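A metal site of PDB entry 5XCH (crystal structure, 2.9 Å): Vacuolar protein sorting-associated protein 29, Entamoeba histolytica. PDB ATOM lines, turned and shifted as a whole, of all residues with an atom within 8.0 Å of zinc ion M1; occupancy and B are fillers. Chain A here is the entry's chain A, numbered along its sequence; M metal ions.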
ATOM      1  N   GLY A   7     -20.540  -8.914 -17.010  1.00  0.00           N
ATOM      2  CA  GLY A   7     -20.859  -8.356 -18.310  1.00  0.00           C
ATOM      3  C   GLY A   7     -19.752  -7.418 -18.790  1.00  0.00           C
ATOM      4  O   GLY A   7     -18.607  -7.529 -18.366  1.00  0.00           O
ATOM      5  N   ASP A   8     -20.130  -6.525 -19.710  1.00  0.00           N
ATOM      6  CA  ASP A   8     -19.292  -5.403 -20.144  1.00  0.00           C
ATOM      7  C   ASP A   8     -17.888  -5.843 -20.574  1.00  0.00           C
ATOM      8  O   ASP A   8     -16.902  -5.184 -20.268  1.00  0.00           O
ATOM      9  CB  ASP A   8     -19.189  -4.336 -19.055  1.00  0.00           C
ATOM     10  CG  ASP A   8     -20.419  -3.456 -18.982  1.00  0.00           C
ATOM     11  OD1 ASP A   8     -20.532  -2.530 -19.812  1.00  0.00           O
ATOM     12  OD2 ASP A   8     -21.258  -3.667 -18.087  1.00  0.00           O
ATOM     13  N   PHE A   9     -17.799  -6.961 -21.300  1.00  0.00           N
ATOM     14  CA  PHE A   9     -16.496  -7.481 -21.660  1.00  0.00           C
ATOM     15  C   PHE A   9     -16.096  -7.165 -23.100  1.00  0.00           C
ATOM     16  O   PHE A   9     -15.114  -7.733 -23.594  1.00  0.00           O
ATOM     17  CB  PHE A   9     -16.434  -8.991 -21.417  1.00  0.00           C
ATOM     18  CG  PHE A   9     -17.725  -9.696 -21.661  1.00  0.00           C
ATOM     19  CD1 PHE A   9     -18.058 -10.121 -22.935  1.00  0.00           C
ATOM     20  CD2 PHE A   9     -18.594  -9.945 -20.622  1.00  0.00           C
ATOM     21  CE1 PHE A   9     -19.235 -10.777 -23.159  1.00  0.00           C
ATOM     22  CE2 PHE A   9     -19.780 -10.598 -20.840  1.00  0.00           C
ATOM     23  CZ  PHE A   9     -20.107 -11.011 -22.112  1.00  0.00           C
ATOM     24  N   HIS A  10     -16.800  -6.272 -23.784  1.00  0.00           N
ATOM     25  CA  HIS A  10     -16.400  -5.934 -25.138  1.00  0.00           C
ATOM     26  C   HIS A  10     -16.697  -4.481 -25.453  1.00  0.00           C
ATOM     27  O   HIS A  10     -17.479  -3.808 -24.773  1.00  0.00           O
ATOM     28  CB  HIS A  10     -17.073  -6.845 -26.175  1.00  0.00           C
ATOM     29  CG  HIS A  10     -16.178  -7.937 -26.670  1.00  0.00           C
ATOM     30  ND1 HIS A  10     -15.740  -8.955 -25.884  1.00  0.00           N
ATOM     31  CD2 HIS A  10     -15.645  -8.170 -27.871  1.00  0.00           C
ATOM     32  CE1 HIS A  10     -14.977  -9.764 -26.585  1.00  0.00           C
ATOM     33  NE2 HIS A  10     -14.903  -9.315 -27.793  1.00  0.00           N
ATOM     34  N   VAL A  11     -16.049  -4.015 -26.519  1.00  0.00           N
ATOM     35  CA  VAL A  11     -16.193  -2.675 -27.077  1.00  0.00           C
ATOM     36  C   VAL A  11     -16.075  -2.849 -28.590  1.00  0.00           C
ATOM     37  O   VAL A  11     -15.662  -3.932 -29.038  1.00  0.00           O
ATOM     38  CB  VAL A  11     -15.137  -1.710 -26.520  1.00  0.00           C
ATOM     39  CG1 VAL A  11     -15.545  -1.216 -25.133  1.00  0.00           C
ATOM     40  CG2 VAL A  11     -13.790  -2.413 -26.436  1.00  0.00           C
ATOM     41  N   PRO A  12     -16.448  -1.869 -29.409  1.00  0.00           N
ATOM     42  CA  PRO A  12     -16.405  -2.075 -30.871  1.00  0.00           C
ATOM     43  C   PRO A  12     -14.986  -2.343 -31.382  1.00  0.00           C
ATOM     44  O   PRO A  12     -14.090  -1.503 -31.243  1.00  0.00           O
ATOM     45  CB  PRO A  12     -16.963  -0.769 -31.427  1.00  0.00           C
ATOM     46  CG  PRO A  12     -17.852  -0.266 -30.355  1.00  0.00           C
ATOM     47  CD  PRO A  12     -17.164  -0.627 -29.071  1.00  0.00           C
ATOM     48  N   THR A  37     -25.228  -7.369 -17.408  1.00  0.00           N
ATOM     49  CA  THR A  37     -25.443  -5.976 -17.757  1.00  0.00           C
ATOM     50  C   THR A  37     -25.391  -5.741 -19.262  1.00  0.00           C
ATOM     51  O   THR A  37     -25.992  -4.788 -19.754  1.00  0.00           O
ATOM     52  CB  THR A  37     -24.420  -5.078 -17.066  1.00  0.00           C
ATOM     53  OG1 THR A  37     -23.130  -5.244 -17.654  1.00  0.00           O
ATOM     54  CG2 THR A  37     -24.349  -5.406 -15.594  1.00  0.00           C
ATOM     55  N   GLY A  38     -24.676  -6.594 -19.998  1.00  0.00           N
ATOM     56  CA  GLY A  38     -24.716  -6.580 -21.446  1.00  0.00           C
ATOM     57  C   GLY A  38     -23.324  -6.403 -22.055  1.00  0.00           C
ATOM     58  O   GLY A  38     -22.327  -6.843 -21.496  1.00  0.00           O
ATOM     59  N   ASN A  39     -23.319  -5.761 -23.216  1.00  0.00           N
ATOM     60  CA  ASN A  39     -22.147  -5.665 -24.093  1.00  0.00           C
ATOM     61  C   ASN A  39     -21.449  -7.019 -24.214  1.00  0.00           C
ATOM     62  O   ASN A  39     -20.278  -7.195 -23.873  1.00  0.00           O
ATOM     63  CB  ASN A  39     -21.177  -4.583 -23.630  1.00  0.00           C
ATOM     64  CG  ASN A  39     -21.043  -3.463 -24.643  1.00  0.00           C
ATOM     65  OD1 ASN A  39     -20.600  -2.362 -24.324  1.00  0.00           O
ATOM     66  ND2 ASN A  39     -21.446  -3.748 -25.883  1.00  0.00           N
ATOM     67  N   LEU A  40     -22.211  -7.987 -24.712  1.00  0.00           N
ATOM     68  CA  LEU A  40     -21.678  -9.318 -24.950  1.00  0.00           C
ATOM     69  C   LEU A  40     -20.748  -9.307 -26.145  1.00  0.00           C
ATOM     70  O   LEU A  40     -20.858  -8.463 -27.045  1.00  0.00           O
ATOM     71  CB  LEU A  40     -22.818 -10.316 -25.182  1.00  0.00           C
ATOM     72  CG  LEU A  40     -23.554 -10.932 -23.989  1.00  0.00           C
ATOM     73  CD1 LEU A  40     -23.458 -10.073 -22.736  1.00  0.00           C
ATOM     74  CD2 LEU A  40     -25.006 -11.177 -24.359  1.00  0.00           C
ATOM     75  N   GLY A  61     -26.763  -2.915 -24.379  1.00  0.00           N
ATOM     76  CA  GLY A  61     -25.854  -1.817 -24.114  1.00  0.00           C
ATOM     77  C   GLY A  61     -25.388  -1.125 -25.382  1.00  0.00           C
ATOM     78  O   GLY A  61     -25.982  -1.314 -26.450  1.00  0.00           O
ATOM     79  N   ASP A  62     -24.308  -0.351 -25.271  1.00  0.00           N
ATOM     80  CA  ASP A  62     -23.871   0.514 -26.360  1.00  0.00           C
ATOM     81  C   ASP A  62     -23.577  -0.283 -27.627  1.00  0.00           C
ATOM     82  O   ASP A  62     -23.937   0.147 -28.739  1.00  0.00           O
ATOM     83  CB  ASP A  62     -22.635   1.301 -25.935  1.00  0.00           C
ATOM     84  CG  ASP A  62     -21.579   0.416 -25.301  1.00  0.00           C
ATOM     85  OD1 ASP A  62     -21.765   0.035 -24.126  1.00  0.00           O
ATOM     86  OD2 ASP A  62     -20.578   0.101 -25.980  1.00  0.00           O
ATOM     87  N   PHE A  63     -22.919  -1.431 -27.507  1.00  0.00           N
ATOM     88  CA  PHE A  63     -22.458  -2.187 -28.666  1.00  0.00           C
ATOM     89  C   PHE A  63     -23.018  -3.601 -28.715  1.00  0.00           C
ATOM     90  O   PHE A  63     -22.353  -4.521 -29.190  1.00  0.00           O
ATOM     91  CB  PHE A  63     -20.927  -2.217 -28.713  1.00  0.00           C
ATOM     92  N   ASP A  64     -24.235  -3.800 -28.221  1.00  0.00           N
ATOM     93  CA  ASP A  64     -24.904  -5.078 -28.370  1.00  0.00           C
ATOM     94  C   ASP A  64     -25.545  -5.173 -29.747  1.00  0.00           C
ATOM     95  O   ASP A  64     -26.064  -4.192 -30.279  1.00  0.00           O
ATOM     96  CB  ASP A  64     -25.966  -5.271 -27.276  1.00  0.00           C
ATOM     97  CG  ASP A  64     -25.363  -5.539 -25.918  1.00  0.00           C
ATOM     98  OD1 ASP A  64     -24.862  -4.578 -25.289  1.00  0.00           O
ATOM     99  OD2 ASP A  64     -25.377  -6.711 -25.479  1.00  0.00           O
ATOM    100  N   HIS A  86     -27.901  -1.554 -18.591  1.00  0.00           N
ATOM    101  CA  HIS A  86     -26.501  -1.375 -18.941  1.00  0.00           C
ATOM    102  C   HIS A  86     -25.945  -0.059 -18.414  1.00  0.00           C
ATOM    103  O   HIS A  86     -24.750   0.022 -18.081  1.00  0.00           O
ATOM    104  CB  HIS A  86     -26.323  -1.443 -20.450  1.00  0.00           C
ATOM    105  CG  HIS A  86     -24.961  -1.880 -20.890  1.00  0.00           C
ATOM    106  ND1 HIS A  86     -24.523  -3.183 -20.772  1.00  0.00           N
ATOM    107  CD2 HIS A  86     -23.939  -1.197 -21.440  1.00  0.00           C
ATOM    108  CE1 HIS A  86     -23.288  -3.272 -21.233  1.00  0.00           C
ATOM    109  NE2 HIS A  86     -22.906  -2.084 -21.643  1.00  0.00           N
ATOM    110  N   GLY A  87     -26.769   0.983 -18.340  1.00  0.00           N
ATOM    111  CA  GLY A  87     -26.319   2.287 -17.915  1.00  0.00           C
ATOM    112  C   GLY A  87     -25.774   3.171 -19.017  1.00  0.00           C
ATOM    113  O   GLY A  87     -25.426   4.327 -18.737  1.00  0.00           O
ATOM    114  N   HIS A  88     -25.689   2.668 -20.251  1.00  0.00           N
ATOM    115  CA  HIS A  88     -25.246   3.511 -21.360  1.00  0.00           C
ATOM    116  C   HIS A  88     -26.249   4.622 -21.656  1.00  0.00           C
ATOM    117  O   HIS A  88     -25.896   5.597 -22.316  1.00  0.00           O
ATOM    118  CB  HIS A  88     -25.020   2.662 -22.613  1.00  0.00           C
ATOM    119  CG  HIS A  88     -26.214   2.547 -23.503  1.00  0.00           C
ATOM    120  ND1 HIS A  88     -26.430   3.391 -24.568  1.00  0.00           N
ATOM    121  CD2 HIS A  88     -27.260   1.695 -23.485  1.00  0.00           C
ATOM    122  CE1 HIS A  88     -27.555   3.067 -25.173  1.00  0.00           C
ATOM    123  NE2 HIS A  88     -28.085   2.030 -24.531  1.00  0.00           N
ATOM    124  N   TRP A  93     -22.829   9.382 -17.093  1.00  0.00           N
ATOM    125  CA  TRP A  93     -22.457   8.042 -16.676  1.00  0.00           C
ATOM    126  C   TRP A  93     -21.907   8.057 -15.251  1.00  0.00           C
ATOM    127  O   TRP A  93     -21.124   8.932 -14.886  1.00  0.00           O
ATOM    128  CB  TRP A  93     -21.423   7.447 -17.631  1.00  0.00           C
ATOM    129  CG  TRP A  93     -21.910   7.311 -19.054  1.00  0.00           C
ATOM    130  CD1 TRP A  93     -23.207   7.352 -19.471  1.00  0.00           C
ATOM    131  CD2 TRP A  93     -21.118   7.120 -20.235  1.00  0.00           C
ATOM    132  NE1 TRP A  93     -23.269   7.195 -20.834  1.00  0.00           N
ATOM    133  CE2 TRP A  93     -22.010   7.055 -21.328  1.00  0.00           C
ATOM    134  CE3 TRP A  93     -19.746   6.999 -20.466  1.00  0.00           C
ATOM    135  CZ2 TRP A  93     -21.559   6.863 -22.638  1.00  0.00           C
ATOM    136  CZ3 TRP A  93     -19.312   6.812 -21.766  1.00  0.00           C
ATOM    137  CH2 TRP A  93     -20.213   6.747 -22.837  1.00  0.00           C
ATOM    138  N   GLY A 114     -23.580  -0.891 -15.646  1.00  0.00           N
ATOM    139  CA  GLY A 114     -22.368  -1.250 -16.358  1.00  0.00           C
ATOM    140  C   GLY A 114     -21.814  -0.026 -17.054  1.00  0.00           C
ATOM    141  O   GLY A 114     -22.245   1.096 -16.768  1.00  0.00           O
ATOM    142  N   HIS A 115     -20.851  -0.225 -17.962  1.00  0.00           N
ATOM    143  CA  HIS A 115     -20.234   0.771 -18.834  1.00  0.00           C
ATOM    144  C   HIS A 115     -19.167   1.594 -18.096  1.00  0.00           C
ATOM    145  O   HIS A 115     -18.436   2.331 -18.761  1.00  0.00           O
ATOM    146  CB  HIS A 115     -21.260   1.723 -19.472  1.00  0.00           C
ATOM    147  CG  HIS A 115     -20.841   2.259 -20.797  1.00  0.00           C
ATOM    148  ND1 HIS A 115     -20.565   1.449 -21.874  1.00  0.00           N
ATOM    149  CD2 HIS A 115     -20.678   3.524 -21.241  1.00  0.00           C
ATOM    150  CE1 HIS A 115     -20.227   2.185 -22.923  1.00  0.00           C
ATOM    151  NE2 HIS A 115     -20.290   3.453 -22.554  1.00  0.00           N
ATOM    152  N   THR A 116     -19.050   1.503 -16.779  1.00  0.00           N
ATOM    153  CA  THR A 116     -17.945   2.134 -16.063  1.00  0.00           C
ATOM    154  C   THR A 116     -16.712   1.250 -15.995  1.00  0.00           C
ATOM    155  O   THR A 116     -15.597   1.766 -15.840  1.00  0.00           O
ATOM    156  CB  THR A 116     -18.361   2.523 -14.638  1.00  0.00           C
ATOM    157  OG1 THR A 116     -19.095   1.443 -14.045  1.00  0.00           O
ATOM    158  CG2 THR A 116     -19.224   3.769 -14.646  1.00  0.00           C
ATOM    159  N   HIS A 117     -16.904  -0.072 -16.085  1.00  0.00           N
ATOM    160  CA  HIS A 117     -15.841  -1.073 -16.054  1.00  0.00           C
ATOM    161  C   HIS A 117     -15.183  -1.204 -14.677  1.00  0.00           C
ATOM    162  O   HIS A 117     -14.078  -1.736 -14.575  1.00  0.00           O
ATOM    163  CB  HIS A 117     -14.764  -0.810 -17.101  1.00  0.00           C
ATOM    164  CG  HIS A 117     -15.192  -1.123 -18.501  1.00  0.00           C
ATOM    165  ND1 HIS A 117     -14.304  -1.240 -19.548  1.00  0.00           N
ATOM    166  CD2 HIS A 117     -16.423  -1.345 -19.034  1.00  0.00           C
ATOM    167  CE1 HIS A 117     -14.969  -1.523 -20.661  1.00  0.00           C
ATOM    168  NE2 HIS A 117     -16.250  -1.593 -20.369  1.00  0.00           N
ATOM    169  N   ALA A 138     -12.070  -5.063 -20.325  1.00  0.00           N
ATOM    170  CA  ALA A 138     -12.146  -4.429 -21.626  1.00  0.00           C
ATOM    171  C   ALA A 138     -11.740  -2.956 -21.541  1.00  0.00           C
ATOM    172  O   ALA A 138     -11.815  -2.321 -20.487  1.00  0.00           O
ATOM    173  CB  ALA A 138     -13.561  -4.548 -22.208  1.00  0.00           C
ATOM    174  N   TYR A 139     -11.311  -2.422 -22.677  1.00  0.00           N
ATOM    175  CA  TYR A 139     -10.790  -1.067 -22.759  1.00  0.00           C
ATOM    176  C   TYR A 139     -11.932  -0.073 -22.947  1.00  0.00           C
ATOM    177  O   TYR A 139     -12.776  -0.236 -23.842  1.00  0.00           O
ATOM    178  CB  TYR A 139      -9.796  -0.966 -23.915  1.00  0.00           C
ATOM    179  CG  TYR A 139      -9.488   0.442 -24.374  1.00  0.00           C
ATOM    180  CD1 TYR A 139      -8.600   1.249 -23.678  1.00  0.00           C
ATOM    181  CD2 TYR A 139     -10.075   0.960 -25.519  1.00  0.00           C
ATOM    182  CE1 TYR A 139      -8.319   2.538 -24.104  1.00  0.00           C
ATOM    183  CE2 TYR A 139      -9.798   2.230 -25.959  1.00  0.00           C
ATOM    184  CZ  TYR A 139      -8.917   3.021 -25.248  1.00  0.00           C
ATOM    185  OH  TYR A 139      -8.634   4.295 -25.682  1.00  0.00           O
ATOM    186  N   SER A 140     -11.962   0.949 -22.104  1.00  0.00           N
ATOM    187  CA  SER A 140     -12.971   1.991 -22.146  1.00  0.00           C
ATOM    188  C   SER A 140     -12.285   3.342 -21.968  1.00  0.00           C
ATOM    189  O   SER A 140     -11.164   3.404 -21.453  1.00  0.00           O
ATOM    190  CB  SER A 140     -14.025   1.787 -21.053  1.00  0.00           C
ATOM    191  OG  SER A 140     -15.117   2.684 -21.214  1.00  0.00           O
ATOM    192  N   LEU A 142     -12.984   5.287 -19.833  1.00  0.00           N
ATOM    193  CA  LEU A 142     -12.916   5.470 -18.378  1.00  0.00           C
ATOM    194  C   LEU A 142     -11.645   4.855 -17.804  1.00  0.00           C
ATOM    195  O   LEU A 142     -10.937   5.496 -17.023  1.00  0.00           O
ATOM    196  CB  LEU A 142     -14.165   4.886 -17.714  1.00  0.00           C
ATOM    197  CG  LEU A 142     -15.524   5.408 -18.094  1.00  0.00           C
ATOM    198  CD1 LEU A 142     -15.547   6.839 -18.256  1.00  0.00           C
ATOM    199  CD2 LEU A 142     -16.088   4.763 -19.298  1.00  0.00           C
HETATM  200 ZN    ZN M   1     -20.096  -0.650 -22.727  1.00  0.00          ZN
HETATM  201 ZN    ZN M   2     -18.512  -1.998 -21.353  1.00  0.00          ZN
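A ring nitrogen (NE2) of His 86 sits close to the side-chain carboxylate (OD1) of Asp 62, at 3.5 Å.
The backbone NH of His 115 sits close to the side-chain carboxylate of Asp 8 (3.5 Å).
The side-chain amide oxygen of Asn 39 lies close to the backbone carbonyl oxygen of His 10 (3.5 Å).
The backbone NH of Phe 63 lies close to the side-chain amide nitrogen of Asn 39, at 3.2 Å.
A ring nitrogen (NE2) of His 86 lies close to the side-chain carboxylate (OD1) of Asp 8, 3.0 Å away.
The backbone carbonyl oxygen (O) of His 86 lies within hydrogen-bond range of the backbone NH (N) of Gly 114 (2.9 Å).
ND1 of His 86 is in hydrogen-bond range of O of Thr 37.
The backbone NH (N) of Asp 8 lies within hydrogen-bond range of the backbone carbonyl oxygen (O) of Gly 38, at 2.8 Å.
Residues that only touch zinc ion M1: Asp 8 (3.5 Å) and His 86 (3.3 Å).
Of the 26 residues printed, 5 come within 4 Å of zinc ion M1.
Zinc ion M1 is bound by OD1 of Asp 62 (2.3 Å), ND1 of His 115 (2.3 Å) and OD1 of Asn 39 (2.4 Å).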
